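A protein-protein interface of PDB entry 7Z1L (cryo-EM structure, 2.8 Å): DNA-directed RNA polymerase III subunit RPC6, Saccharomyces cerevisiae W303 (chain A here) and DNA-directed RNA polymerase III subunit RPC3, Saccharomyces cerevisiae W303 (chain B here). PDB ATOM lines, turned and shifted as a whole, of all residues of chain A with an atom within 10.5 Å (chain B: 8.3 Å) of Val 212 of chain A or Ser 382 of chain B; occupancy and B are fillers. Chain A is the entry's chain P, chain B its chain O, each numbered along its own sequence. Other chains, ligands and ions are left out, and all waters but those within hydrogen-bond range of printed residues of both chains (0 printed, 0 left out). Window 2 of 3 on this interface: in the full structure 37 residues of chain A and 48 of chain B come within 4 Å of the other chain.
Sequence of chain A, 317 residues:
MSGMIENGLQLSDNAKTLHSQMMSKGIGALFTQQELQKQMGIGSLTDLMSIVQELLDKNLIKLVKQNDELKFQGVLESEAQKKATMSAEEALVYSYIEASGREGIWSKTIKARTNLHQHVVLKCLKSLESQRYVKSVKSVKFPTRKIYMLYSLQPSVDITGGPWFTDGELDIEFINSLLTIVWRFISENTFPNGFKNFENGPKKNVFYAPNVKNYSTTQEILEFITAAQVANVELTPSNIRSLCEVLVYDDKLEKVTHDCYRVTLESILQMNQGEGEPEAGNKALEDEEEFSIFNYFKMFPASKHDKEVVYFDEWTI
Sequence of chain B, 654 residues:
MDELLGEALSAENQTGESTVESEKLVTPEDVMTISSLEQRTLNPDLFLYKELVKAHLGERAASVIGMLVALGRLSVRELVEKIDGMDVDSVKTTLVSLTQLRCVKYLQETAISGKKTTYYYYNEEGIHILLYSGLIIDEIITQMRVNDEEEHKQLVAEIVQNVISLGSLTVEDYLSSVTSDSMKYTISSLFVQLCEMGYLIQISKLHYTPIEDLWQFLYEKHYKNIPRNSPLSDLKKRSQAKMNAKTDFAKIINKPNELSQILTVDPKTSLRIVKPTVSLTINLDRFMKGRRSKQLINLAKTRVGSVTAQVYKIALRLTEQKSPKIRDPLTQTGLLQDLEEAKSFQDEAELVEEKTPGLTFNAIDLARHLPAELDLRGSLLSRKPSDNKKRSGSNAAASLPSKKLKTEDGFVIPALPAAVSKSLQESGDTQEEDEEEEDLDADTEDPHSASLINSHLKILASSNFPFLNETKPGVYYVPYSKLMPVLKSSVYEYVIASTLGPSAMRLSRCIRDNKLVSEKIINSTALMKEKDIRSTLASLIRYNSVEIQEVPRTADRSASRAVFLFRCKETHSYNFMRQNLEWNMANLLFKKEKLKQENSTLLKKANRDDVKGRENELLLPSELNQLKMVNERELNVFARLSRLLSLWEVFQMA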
ATOM      1  N   GLU A 188      16.112 -12.308   6.193  1.00  0.00           N
ATOM      2  CA  GLU A 188      17.110 -11.255   6.026  1.00  0.00           C
ATOM      3  C   GLU A 188      16.664 -10.221   5.004  1.00  0.00           C
ATOM      4  O   GLU A 188      16.871  -9.019   5.204  1.00  0.00           O
ATOM      5  CB  GLU A 188      18.466 -11.842   5.626  1.00  0.00           C
ATOM      6  CG  GLU A 188      19.148 -12.702   6.680  1.00  0.00           C
ATOM      7  CD  GLU A 188      19.575 -11.901   7.893  1.00  0.00           C
ATOM      8  OE1 GLU A 188      19.909 -10.710   7.724  1.00  0.00           O
ATOM      9  OE2 GLU A 188      19.593 -12.462   9.012  1.00  0.00           O
ATOM     10  N   ASN A 189      16.055 -10.659   3.899  1.00  0.00           N
ATOM     11  CA  ASN A 189      15.668  -9.693   2.871  1.00  0.00           C
ATOM     12  C   ASN A 189      14.444  -8.869   3.271  1.00  0.00           C
ATOM     13  O   ASN A 189      14.368  -7.676   2.958  1.00  0.00           O
ATOM     14  CB  ASN A 189      15.416 -10.387   1.533  1.00  0.00           C
ATOM     15  CG  ASN A 189      16.659 -11.035   0.970  1.00  0.00           C
ATOM     16  OD1 ASN A 189      17.620 -10.356   0.624  1.00  0.00           O
ATOM     17  ND2 ASN A 189      16.648 -12.359   0.878  1.00  0.00           N
ATOM     18  N   THR A 190      13.477  -9.479   3.956  1.00  0.00           N
ATOM     19  CA  THR A 190      12.192  -8.827   4.194  1.00  0.00           C
ATOM     20  C   THR A 190      12.196  -7.885   5.390  1.00  0.00           C
ATOM     21  O   THR A 190      11.169  -7.256   5.663  1.00  0.00           O
ATOM     22  CB  THR A 190      11.081  -9.862   4.393  1.00  0.00           C
ATOM     23  OG1 THR A 190       9.818  -9.190   4.446  1.00  0.00           O
ATOM     24  CG2 THR A 190      11.276 -10.599   5.701  1.00  0.00           C
ATOM     25  N   PHE A 191      13.306  -7.771   6.109  1.00  0.00           N
ATOM     26  CA  PHE A 191      13.347  -6.915   7.280  1.00  0.00           C
ATOM     27  C   PHE A 191      14.511  -5.937   7.177  1.00  0.00           C
ATOM     28  O   PHE A 191      15.496  -6.216   6.485  1.00  0.00           O
ATOM     29  CB  PHE A 191      13.465  -7.753   8.560  1.00  0.00           C
ATOM     30  CG  PHE A 191      12.170  -8.379   8.987  1.00  0.00           C
ATOM     31  CD1 PHE A 191      11.064  -7.590   9.263  1.00  0.00           C
ATOM     32  CD2 PHE A 191      12.049  -9.753   9.096  1.00  0.00           C
ATOM     33  CE1 PHE A 191       9.865  -8.160   9.651  1.00  0.00           C
ATOM     34  CE2 PHE A 191      10.852 -10.328   9.479  1.00  0.00           C
ATOM     35  CZ  PHE A 191       9.760  -9.530   9.758  1.00  0.00           C
ATOM     36  N   PRO A 192      14.412  -4.767   7.825  1.00  0.00           N
ATOM     37  CA  PRO A 192      15.475  -3.754   7.662  1.00  0.00           C
ATOM     38  C   PRO A 192      16.842  -4.209   8.146  1.00  0.00           C
ATOM     39  O   PRO A 192      17.814  -4.158   7.381  1.00  0.00           O
ATOM     40  CB  PRO A 192      14.941  -2.571   8.482  1.00  0.00           C
ATOM     41  CG  PRO A 192      13.466  -2.748   8.475  1.00  0.00           C
ATOM     42  CD  PRO A 192      13.253  -4.226   8.557  1.00  0.00           C
ATOM     43  N   VAL A 206      11.973  -1.860  13.916  1.00  0.00           N
ATOM     44  CA  VAL A 206      11.464  -1.020  12.841  1.00  0.00           C
ATOM     45  C   VAL A 206      11.075  -1.909  11.668  1.00  0.00           C
ATOM     46  O   VAL A 206      11.488  -3.067  11.567  1.00  0.00           O
ATOM     47  CB  VAL A 206      12.485   0.048  12.393  1.00  0.00           C
ATOM     48  CG1 VAL A 206      12.814   0.996  13.535  1.00  0.00           C
ATOM     49  CG2 VAL A 206      13.747  -0.614  11.863  1.00  0.00           C
ATOM     50  N   PHE A 207      10.265  -1.350  10.775  1.00  0.00           N
ATOM     51  CA  PHE A 207       9.751  -2.067   9.619  1.00  0.00           C
ATOM     52  C   PHE A 207       9.855  -1.197   8.373  1.00  0.00           C
ATOM     53  O   PHE A 207       9.951   0.031   8.445  1.00  0.00           O
ATOM     54  CB  PHE A 207       8.301  -2.505   9.852  1.00  0.00           C
ATOM     55  CG  PHE A 207       8.148  -3.516  10.949  1.00  0.00           C
ATOM     56  CD1 PHE A 207       8.307  -4.867  10.692  1.00  0.00           C
ATOM     57  CD2 PHE A 207       7.867  -3.113  12.243  1.00  0.00           C
ATOM     58  CE1 PHE A 207       8.172  -5.798  11.703  1.00  0.00           C
ATOM     59  CE2 PHE A 207       7.737  -4.037  13.258  1.00  0.00           C
ATOM     60  CZ  PHE A 207       7.888  -5.381  12.988  1.00  0.00           C
ATOM     61  N   TYR A 208       9.837  -1.855   7.217  1.00  0.00           N
ATOM     62  CA  TYR A 208       9.934  -1.157   5.946  1.00  0.00           C
ATOM     63  C   TYR A 208       8.649  -0.393   5.641  1.00  0.00           C
ATOM     64  O   TYR A 208       7.568  -0.706   6.144  1.00  0.00           O
ATOM     65  CB  TYR A 208      10.224  -2.138   4.810  1.00  0.00           C
ATOM     66  CG  TYR A 208      11.678  -2.525   4.668  1.00  0.00           C
ATOM     67  CD1 TYR A 208      12.682  -1.570   4.752  1.00  0.00           C
ATOM     68  CD2 TYR A 208      12.044  -3.843   4.434  1.00  0.00           C
ATOM     69  CE1 TYR A 208      14.012  -1.921   4.616  1.00  0.00           C
ATOM     70  CE2 TYR A 208      13.369  -4.202   4.297  1.00  0.00           C
ATOM     71  CZ  TYR A 208      14.349  -3.237   4.387  1.00  0.00           C
ATOM     72  OH  TYR A 208      15.671  -3.591   4.251  1.00  0.00           O
ATOM     73  N   ALA A 209       8.788   0.628   4.799  1.00  0.00           N
ATOM     74  CA  ALA A 209       7.642   1.365   4.305  1.00  0.00           C
ATOM     75  C   ALA A 209       6.851   0.497   3.326  1.00  0.00           C
ATOM     76  O   ALA A 209       7.394  -0.449   2.749  1.00  0.00           O
ATOM     77  CB  ALA A 209       8.102   2.663   3.641  1.00  0.00           C
ATOM     78  N   PRO A 210       5.553   0.778   3.148  1.00  0.00           N
ATOM     79  CA  PRO A 210       4.745  -0.048   2.232  1.00  0.00           C
ATOM     80  C   PRO A 210       5.229  -0.048   0.792  1.00  0.00           C
ATOM     81  O   PRO A 210       5.036  -1.047   0.089  1.00  0.00           O
ATOM     82  CB  PRO A 210       3.342   0.567   2.352  1.00  0.00           C
ATOM     83  CG  PRO A 210       3.551   1.911   2.982  1.00  0.00           C
ATOM     84  CD  PRO A 210       4.714   1.732   3.891  1.00  0.00           C
ATOM     85  N   ASN A 211       5.848   1.037   0.324  1.00  0.00           N
ATOM     86  CA  ASN A 211       6.322   1.078  -1.054  1.00  0.00           C
ATOM     87  C   ASN A 211       7.630   0.321  -1.254  1.00  0.00           C
ATOM     88  O   ASN A 211       8.024   0.088  -2.402  1.00  0.00           O
ATOM     89  CB  ASN A 211       6.486   2.529  -1.517  1.00  0.00           C
ATOM     90  CG  ASN A 211       7.320   3.362  -0.561  1.00  0.00           C
ATOM     91  OD1 ASN A 211       7.889   2.848   0.398  1.00  0.00           O
ATOM     92  ND2 ASN A 211       7.393   4.661  -0.824  1.00  0.00           N
ATOM     93  N   VAL A 212       8.306  -0.064  -0.173  1.00  0.00           N
ATOM     94  CA  VAL A 212       9.564  -0.791  -0.289  1.00  0.00           C
ATOM     95  C   VAL A 212       9.289  -2.217  -0.742  1.00  0.00           C
ATOM     96  O   VAL A 212       8.399  -2.895  -0.213  1.00  0.00           O
ATOM     97  CB  VAL A 212      10.327  -0.773   1.043  1.00  0.00           C
ATOM     98  CG1 VAL A 212      11.737  -1.303   0.852  1.00  0.00           C
ATOM     99  CG2 VAL A 212      10.364   0.630   1.603  1.00  0.00           C
ATOM    100  N   LYS A 213      10.058  -2.681  -1.728  1.00  0.00           N
ATOM    101  CA  LYS A 213       9.933  -4.045  -2.237  1.00  0.00           C
ATOM    102  C   LYS A 213      10.684  -4.982  -1.294  1.00  0.00           C
ATOM    103  O   LYS A 213      11.804  -5.429  -1.559  1.00  0.00           O
ATOM    104  CB  LYS A 213      10.461  -4.137  -3.663  1.00  0.00           C
ATOM    105  CG  LYS A 213       9.617  -3.396  -4.687  1.00  0.00           C
ATOM    106  CD  LYS A 213      10.065  -3.716  -6.103  1.00  0.00           C
ATOM    107  CE  LYS A 213      11.491  -3.248  -6.346  1.00  0.00           C
ATOM    108  NZ  LYS A 213      11.927  -3.499  -7.748  1.00  0.00           N
ATOM    109  N   ASN A 214      10.046  -5.280  -0.163  1.00  0.00           N
ATOM    110  CA  ASN A 214      10.617  -6.191   0.818  1.00  0.00           C
ATOM    111  C   ASN A 214      10.410  -7.659   0.466  1.00  0.00           C
ATOM    112  O   ASN A 214      11.023  -8.524   1.100  1.00  0.00           O
ATOM    113  CB  ASN A 214      10.042  -5.890   2.209  1.00  0.00           C
ATOM    114  CG  ASN A 214       8.523  -5.985   2.260  1.00  0.00           C
ATOM    115  OD1 ASN A 214       7.870  -6.368   1.290  1.00  0.00           O
ATOM    116  ND2 ASN A 214       7.955  -5.629   3.407  1.00  0.00           N
ATOM    117  N   TYR A 215       9.572  -7.958  -0.522  1.00  0.00           N
ATOM    118  CA  TYR A 215       9.357  -9.336  -0.935  1.00  0.00           C
ATOM    119  C   TYR A 215      10.574  -9.874  -1.678  1.00  0.00           C
ATOM    120  O   TYR A 215      11.300  -9.137  -2.348  1.00  0.00           O
ATOM    121  CB  TYR A 215       8.111  -9.442  -1.816  1.00  0.00           C
ATOM    122  CG  TYR A 215       8.193  -8.678  -3.121  1.00  0.00           C
ATOM    123  CD1 TYR A 215       7.877  -7.327  -3.178  1.00  0.00           C
ATOM    124  CD2 TYR A 215       8.575  -9.310  -4.297  1.00  0.00           C
ATOM    125  CE1 TYR A 215       7.947  -6.626  -4.366  1.00  0.00           C
ATOM    126  CE2 TYR A 215       8.648  -8.616  -5.490  1.00  0.00           C
ATOM    127  CZ  TYR A 215       8.332  -7.276  -5.519  1.00  0.00           C
ATOM    128  OH  TYR A 215       8.404  -6.581  -6.704  1.00  0.00           O
ATOM    129  N   SER A 216      10.791 -11.180  -1.551  1.00  0.00           N
ATOM    130  CA  SER A 216      11.888 -11.871  -2.213  1.00  0.00           C
ATOM    131  C   SER A 216      11.332 -12.745  -3.326  1.00  0.00           C
ATOM    132  O   SER A 216      10.410 -13.535  -3.097  1.00  0.00           O
ATOM    133  CB  SER A 216      12.676 -12.724  -1.220  1.00  0.00           C
ATOM    134  OG  SER A 216      13.156 -11.936  -0.149  1.00  0.00           O
ATOM    135  N   VAL A 256       2.538 -12.899  -1.531  1.00  0.00           N
ATOM    136  CA  VAL A 256       1.813 -11.669  -1.832  1.00  0.00           C
ATOM    137  C   VAL A 256       1.614 -11.570  -3.340  1.00  0.00           C
ATOM    138  O   VAL A 256       0.655 -10.951  -3.816  1.00  0.00           O
ATOM    139  CB  VAL A 256       2.551 -10.441  -1.257  1.00  0.00           C
ATOM    140  CG1 VAL A 256       3.909 -10.242  -1.924  1.00  0.00           C
ATOM    141  CG2 VAL A 256       1.694  -9.182  -1.363  1.00  0.00           C
ATOM    142  N   THR A 257       2.507 -12.202  -4.097  1.00  0.00           N
ATOM    143  CA  THR A 257       2.432 -12.234  -5.550  1.00  0.00           C
ATOM    144  C   THR A 257       3.037 -13.560  -5.989  1.00  0.00           C
ATOM    145  O   THR A 257       3.812 -14.173  -5.251  1.00  0.00           O
ATOM    146  CB  THR A 257       3.166 -11.027  -6.173  1.00  0.00           C
ATOM    147  OG1 THR A 257       2.715  -9.818  -5.549  1.00  0.00           O
ATOM    148  CG2 THR A 257       2.890 -10.903  -7.670  1.00  0.00           C
ATOM    149  N   TYR A 261       7.504 -13.886  -2.092  1.00  0.00           N
ATOM    150  CA  TYR A 261       7.185 -14.311  -0.736  1.00  0.00           C
ATOM    151  C   TYR A 261       7.799 -13.347   0.272  1.00  0.00           C
ATOM    152  O   TYR A 261       8.665 -12.533  -0.057  1.00  0.00           O
ATOM    153  CB  TYR A 261       7.651 -15.747  -0.453  1.00  0.00           C
ATOM    154  CG  TYR A 261       7.372 -16.743  -1.562  1.00  0.00           C
ATOM    155  CD1 TYR A 261       6.265 -17.580  -1.502  1.00  0.00           C
ATOM    156  CD2 TYR A 261       8.243 -16.887  -2.635  1.00  0.00           C
ATOM    157  CE1 TYR A 261       6.010 -18.500  -2.499  1.00  0.00           C
ATOM    158  CE2 TYR A 261       7.996 -17.805  -3.637  1.00  0.00           C
ATOM    159  CZ  TYR A 261       6.880 -18.610  -3.562  1.00  0.00           C
ATOM    160  OH  TYR A 261       6.631 -19.527  -4.555  1.00  0.00           O
ATOM    161  N   ARG A 262       7.331 -13.452   1.515  1.00  0.00           N
ATOM    162  CA  ARG A 262       7.729 -12.538   2.579  1.00  0.00           C
ATOM    163  C   ARG A 262       7.486 -13.201   3.930  1.00  0.00           C
ATOM    164  O   ARG A 262       6.402 -13.729   4.172  1.00  0.00           O
ATOM    165  CB  ARG A 262       6.947 -11.223   2.480  1.00  0.00           C
ATOM    166  CG  ARG A 262       6.858 -10.436   3.772  1.00  0.00           C
ATOM    167  CD  ARG A 262       6.625  -8.961   3.498  1.00  0.00           C
ATOM    168  NE  ARG A 262       5.216  -8.670   3.262  1.00  0.00           N
ATOM    169  CZ  ARG A 262       4.672  -8.519   2.063  1.00  0.00           C
ATOM    170  NH1 ARG A 262       5.393  -8.622   0.959  1.00  0.00           N
ATOM    171  NH2 ARG A 262       3.372  -8.258   1.969  1.00  0.00           N
ATOM    172  N   ARG B 377       7.604   8.195  15.279  1.00  0.00           N
ATOM    173  CA  ARG B 377       8.625   8.946  14.548  1.00  0.00           C
ATOM    174  C   ARG B 377       9.556   8.026  13.765  1.00  0.00           C
ATOM    175  O   ARG B 377       9.613   8.080  12.531  1.00  0.00           O
ATOM    176  CB  ARG B 377       9.426   9.817  15.516  1.00  0.00           C
ATOM    177  CG  ARG B 377       8.639  10.958  16.141  1.00  0.00           C
ATOM    178  CD  ARG B 377       9.515  11.765  17.086  1.00  0.00           C
ATOM    179  NE  ARG B 377       8.798  12.884  17.685  1.00  0.00           N
ATOM    180  CZ  ARG B 377       8.132  12.821  18.829  1.00  0.00           C
ATOM    181  NH1 ARG B 377       8.070  11.702  19.533  1.00  0.00           N
ATOM    182  NH2 ARG B 377       7.515  13.909  19.282  1.00  0.00           N
ATOM    183  N   GLY B 378      10.297   7.176  14.465  1.00  0.00           N
ATOM    184  CA  GLY B 378      11.285   6.328  13.838  1.00  0.00           C
ATOM    185  C   GLY B 378      10.830   4.925  13.514  1.00  0.00           C
ATOM    186  O   GLY B 378      11.673   4.057  13.266  1.00  0.00           O
ATOM    187  N   SER B 379       9.520   4.668  13.505  1.00  0.00           N
ATOM    188  CA  SER B 379       9.027   3.310  13.308  1.00  0.00           C
ATOM    189  C   SER B 379       9.131   2.846  11.862  1.00  0.00           C
ATOM    190  O   SER B 379       9.013   1.645  11.603  1.00  0.00           O
ATOM    191  CB  SER B 379       7.577   3.210  13.779  1.00  0.00           C
ATOM    192  OG  SER B 379       7.444   3.664  15.115  1.00  0.00           O
ATOM    193  N   LEU B 380       9.345   3.757  10.916  1.00  0.00           N
ATOM    194  CA  LEU B 380       9.378   3.419   9.500  1.00  0.00           C
ATOM    195  C   LEU B 380      10.734   3.760   8.903  1.00  0.00           C
ATOM    196  O   LEU B 380      11.294   4.828   9.173  1.00  0.00           O
ATOM    197  CB  LEU B 380       8.282   4.153   8.716  1.00  0.00           C
ATOM    198  CG  LEU B 380       6.920   3.472   8.567  1.00  0.00           C
ATOM    199  CD1 LEU B 380       7.060   2.154   7.830  1.00  0.00           C
ATOM    200  CD2 LEU B 380       6.254   3.264   9.904  1.00  0.00           C
ATOM    201  N   LEU B 381      11.251   2.848   8.087  1.00  0.00           N
ATOM    202  CA  LEU B 381      12.454   3.077   7.297  1.00  0.00           C
ATOM    203  C   LEU B 381      12.035   3.195   5.838  1.00  0.00           C
ATOM    204  O   LEU B 381      11.424   2.272   5.289  1.00  0.00           O
ATOM    205  CB  LEU B 381      13.463   1.946   7.493  1.00  0.00           C
ATOM    206  CG  LEU B 381      14.800   2.099   6.768  1.00  0.00           C
ATOM    207  CD1 LEU B 381      15.546   3.325   7.271  1.00  0.00           C
ATOM    208  CD2 LEU B 381      15.645   0.847   6.934  1.00  0.00           C
ATOM    209  N   SER B 382      12.362   4.330   5.217  1.00  0.00           N
ATOM    210  CA  SER B 382      11.813   4.638   3.901  1.00  0.00           C
ATOM    211  C   SER B 382      12.485   3.842   2.789  1.00  0.00           C
ATOM    212  O   SER B 382      11.849   3.550   1.771  1.00  0.00           O
ATOM    213  CB  SER B 382      11.930   6.136   3.624  1.00  0.00           C
ATOM    214  OG  SER B 382      11.181   6.886   4.563  1.00  0.00           O
ATOM    215  N   ARG B 383      13.759   3.493   2.950  1.00  0.00           N
ATOM    216  CA  ARG B 383      14.501   2.823   1.892  1.00  0.00           C
ATOM    217  C   ARG B 383      15.432   1.779   2.489  1.00  0.00           C
ATOM    218  O   ARG B 383      15.805   1.853   3.662  1.00  0.00           O
ATOM    219  CB  ARG B 383      15.299   3.829   1.054  1.00  0.00           C
ATOM    220  CG  ARG B 383      16.401   4.535   1.822  1.00  0.00           C
ATOM    221  CD  ARG B 383      17.165   5.493   0.927  1.00  0.00           C
ATOM    222  NE  ARG B 383      16.312   6.573   0.446  1.00  0.00           N
ATOM    223  CZ  ARG B 383      16.111   7.713   1.093  1.00  0.00           C
ATOM    224  NH1 ARG B 383      16.681   7.955   2.262  1.00  0.00           N
ATOM    225  NH2 ARG B 383      15.314   8.633   0.555  1.00  0.00           N
ATOM    226  N   LYS B 384      15.803   0.804   1.664  1.00  0.00           N
ATOM    227  CA  LYS B 384      16.691  -0.273   2.089  1.00  0.00           C
ATOM    228  C   LYS B 384      18.116   0.229   2.294  1.00  0.00           C
ATOM    229  O   LYS B 384      19.015  -0.543   2.629  1.00  0.00           O
ATOM    230  CB  LYS B 384      16.680  -1.408   1.064  1.00  0.00           C
ATOM    231  CG  LYS B 384      15.380  -2.195   1.025  1.00  0.00           C
ATOM    232  CD  LYS B 384      15.423  -3.277  -0.040  1.00  0.00           C
ATOM    233  CE  LYS B 384      16.365  -4.402   0.353  1.00  0.00           C
ATOM    234  NZ  LYS B 384      15.886  -5.134   1.558  1.00  0.00           N
ATOM    235  N   LEU B 452       2.820   9.738   8.602  1.00  0.00           N
ATOM    236  CA  LEU B 452       3.226   8.477   9.215  1.00  0.00           C
ATOM    237  C   LEU B 452       2.014   7.628   9.592  1.00  0.00           C
ATOM    238  O   LEU B 452       2.044   6.396   9.465  1.00  0.00           O
ATOM    239  CB  LEU B 452       4.103   8.765  10.432  1.00  0.00           C
ATOM    240  CG  LEU B 452       5.592   8.863  10.092  1.00  0.00           C
ATOM    241  CD1 LEU B 452       6.372   9.483  11.236  1.00  0.00           C
ATOM    242  CD2 LEU B 452       6.153   7.495   9.736  1.00  0.00           C
ATOM    243  N   SER B 455       0.956   6.095   6.460  1.00  0.00           N
ATOM    244  CA  SER B 455       1.836   4.976   6.133  1.00  0.00           C
ATOM    245  C   SER B 455       1.465   3.726   6.925  1.00  0.00           C
ATOM    246  O   SER B 455       1.475   2.612   6.386  1.00  0.00           O
ATOM    247  CB  SER B 455       3.292   5.361   6.391  1.00  0.00           C
ATOM    248  OG  SER B 455       3.623   6.571   5.732  1.00  0.00           O
ATOM    249  N   ILE B 459       0.200   0.222   5.256  1.00  0.00           N
ATOM    250  CA  ILE B 459       0.783  -1.101   5.471  1.00  0.00           C
ATOM    251  C   ILE B 459      -0.233  -2.029   6.131  1.00  0.00           C
ATOM    252  O   ILE B 459      -0.148  -3.255   5.989  1.00  0.00           O
ATOM    253  CB  ILE B 459       2.101  -1.002   6.271  1.00  0.00           C
ATOM    254  CG1 ILE B 459       2.869  -2.324   6.221  1.00  0.00           C
ATOM    255  CG2 ILE B 459       1.852  -0.629   7.715  1.00  0.00           C
ATOM    256  CD1 ILE B 459       3.368  -2.688   4.841  1.00  0.00           C
ATOM    257  N   SER B 462      -2.230  -3.001   2.979  1.00  0.00           N
ATOM    258  CA  SER B 462      -1.441  -3.743   2.006  1.00  0.00           C
ATOM    259  C   SER B 462      -0.955  -5.087   2.531  1.00  0.00           C
ATOM    260  O   SER B 462      -0.226  -5.784   1.820  1.00  0.00           O
ATOM    261  CB  SER B 462      -0.239  -2.908   1.550  1.00  0.00           C
ATOM    262  OG  SER B 462       0.720  -3.716   0.891  1.00  0.00           O
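The backbone NH of Leu 381 of chain B lies within hydrogen-bond range of the backbone carbonyl oxygen of Phe 207 of chain A, at 3.1 Å.
OH of Tyr 208 of chain A is in hydrogen-bond range of NZ of Lys 384 of chain B (3.1 Å).
The backbone carbonyl oxygen (O) of Leu 381 of chain B lies within hydrogen-bond range of the backbone NH (N) of Ala 209 of chain A, 3.1 Å away.
The backbone NH (N) of Phe 207 of chain A lies within hydrogen-bond range of the backbone carbonyl oxygen (O) of Ser 379 of chain B (3.4 Å).
NZ of Lys 384 of chain B sits at hydrogen-bond distance from O of Asn 189 of chain A (3.3 Å).
OH of Tyr 208 of chain A is in hydrogen-bond range of O of Phe 191 of chain A (3.5 Å).
Among the printed residues, merely in contact across the chains: Val 206 of chain A with Gly 378 of chain B (3.3 Å), Val 212 of chain A with Ser 382 of chain B (3.3 Å), Tyr 208 of chain A with Leu 380 of chain B (3.4 Å), Phe 207 of chain A with Leu 380 of chain B (3.6 Å), Ala 209 of chain A with Leu 380 of chain B (3.7 Å), Val 212 of chain A with Lys 384 of chain B (3.8 Å), Tyr 208 of chain A with Leu 381 of chain B (3.8 Å), Pro 192 of chain A with Leu 381 of chain B (3.8 Å), Val 206 of chain A with Ser 379 of chain B (3.8 Å) and Pro 210 of chain A with Ile 459 of chain B (3.96 Å).
Printed residues of chain B within 4 Å of Asn 189 of chain A: Lys 384.
Of the printed residues of chain B, Tyr 208 of chain A touches Leu 380 (3.4 Å), Leu 381 (3.8 Å) and Lys 384 (3.1 Å).
Ala 209 of chain A touches just these residues of chain B: Leu 380 (3.7 Å) and Leu 381 (3.1 Å).
Val 212 of chain A touches just these residues of chain B: Ser 382 and Lys 384.
Of chain A, only Pro 192, Phe 207, Tyr 208 and Ala 209 come within 4 Å of Leu 381 of chain B.
Ser 382 of chain B touches just one residue of chain A: Val 212.
No residue of chain A comes within 4 Å of Arg 383 of chain B.
Ser 455 of chain B touches none of the printed residues of chain A.
The nearest residue of chain B that does not touch Val 212 of chain A is Leu 381 of chain B (4.2 Å).
The nearest residue of chain A that does not touch Ser 382 of chain B is Ala 209 of chain A (4.2 Å).
Of the 12 printed residues of chain B, 7 touch a printed residue of chain A.
Printed residues of chain B that touch a printed residue of chain A: Gly 378, Ser 379, Leu 380, Leu 381, Ser 382, Lys 384 and Ile 459.
Hydrophobic or aromatic side chains of chain B that line the printed part of chain A: Leu 380, Leu 381 and Ile 459.
Along chain B the printed residues that touch a printed residue of chain A span positions 378 to 459.
Of the 20 printed residues of chain A, 8 touch a printed residue of chain B.
Hydrophobic or aromatic side chains of chain A that line the printed part of chain B: Pro 192, Val 206, Tyr 208, Ala 209 and Val 212.
Along chain A the printed residues that touch a printed residue of chain B span positions 189 to 212.
Among the printed residues, no Asp or Glu carboxylate lies within 4 Å of a Lys or Arg side-chain nitrogen of the other chain.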
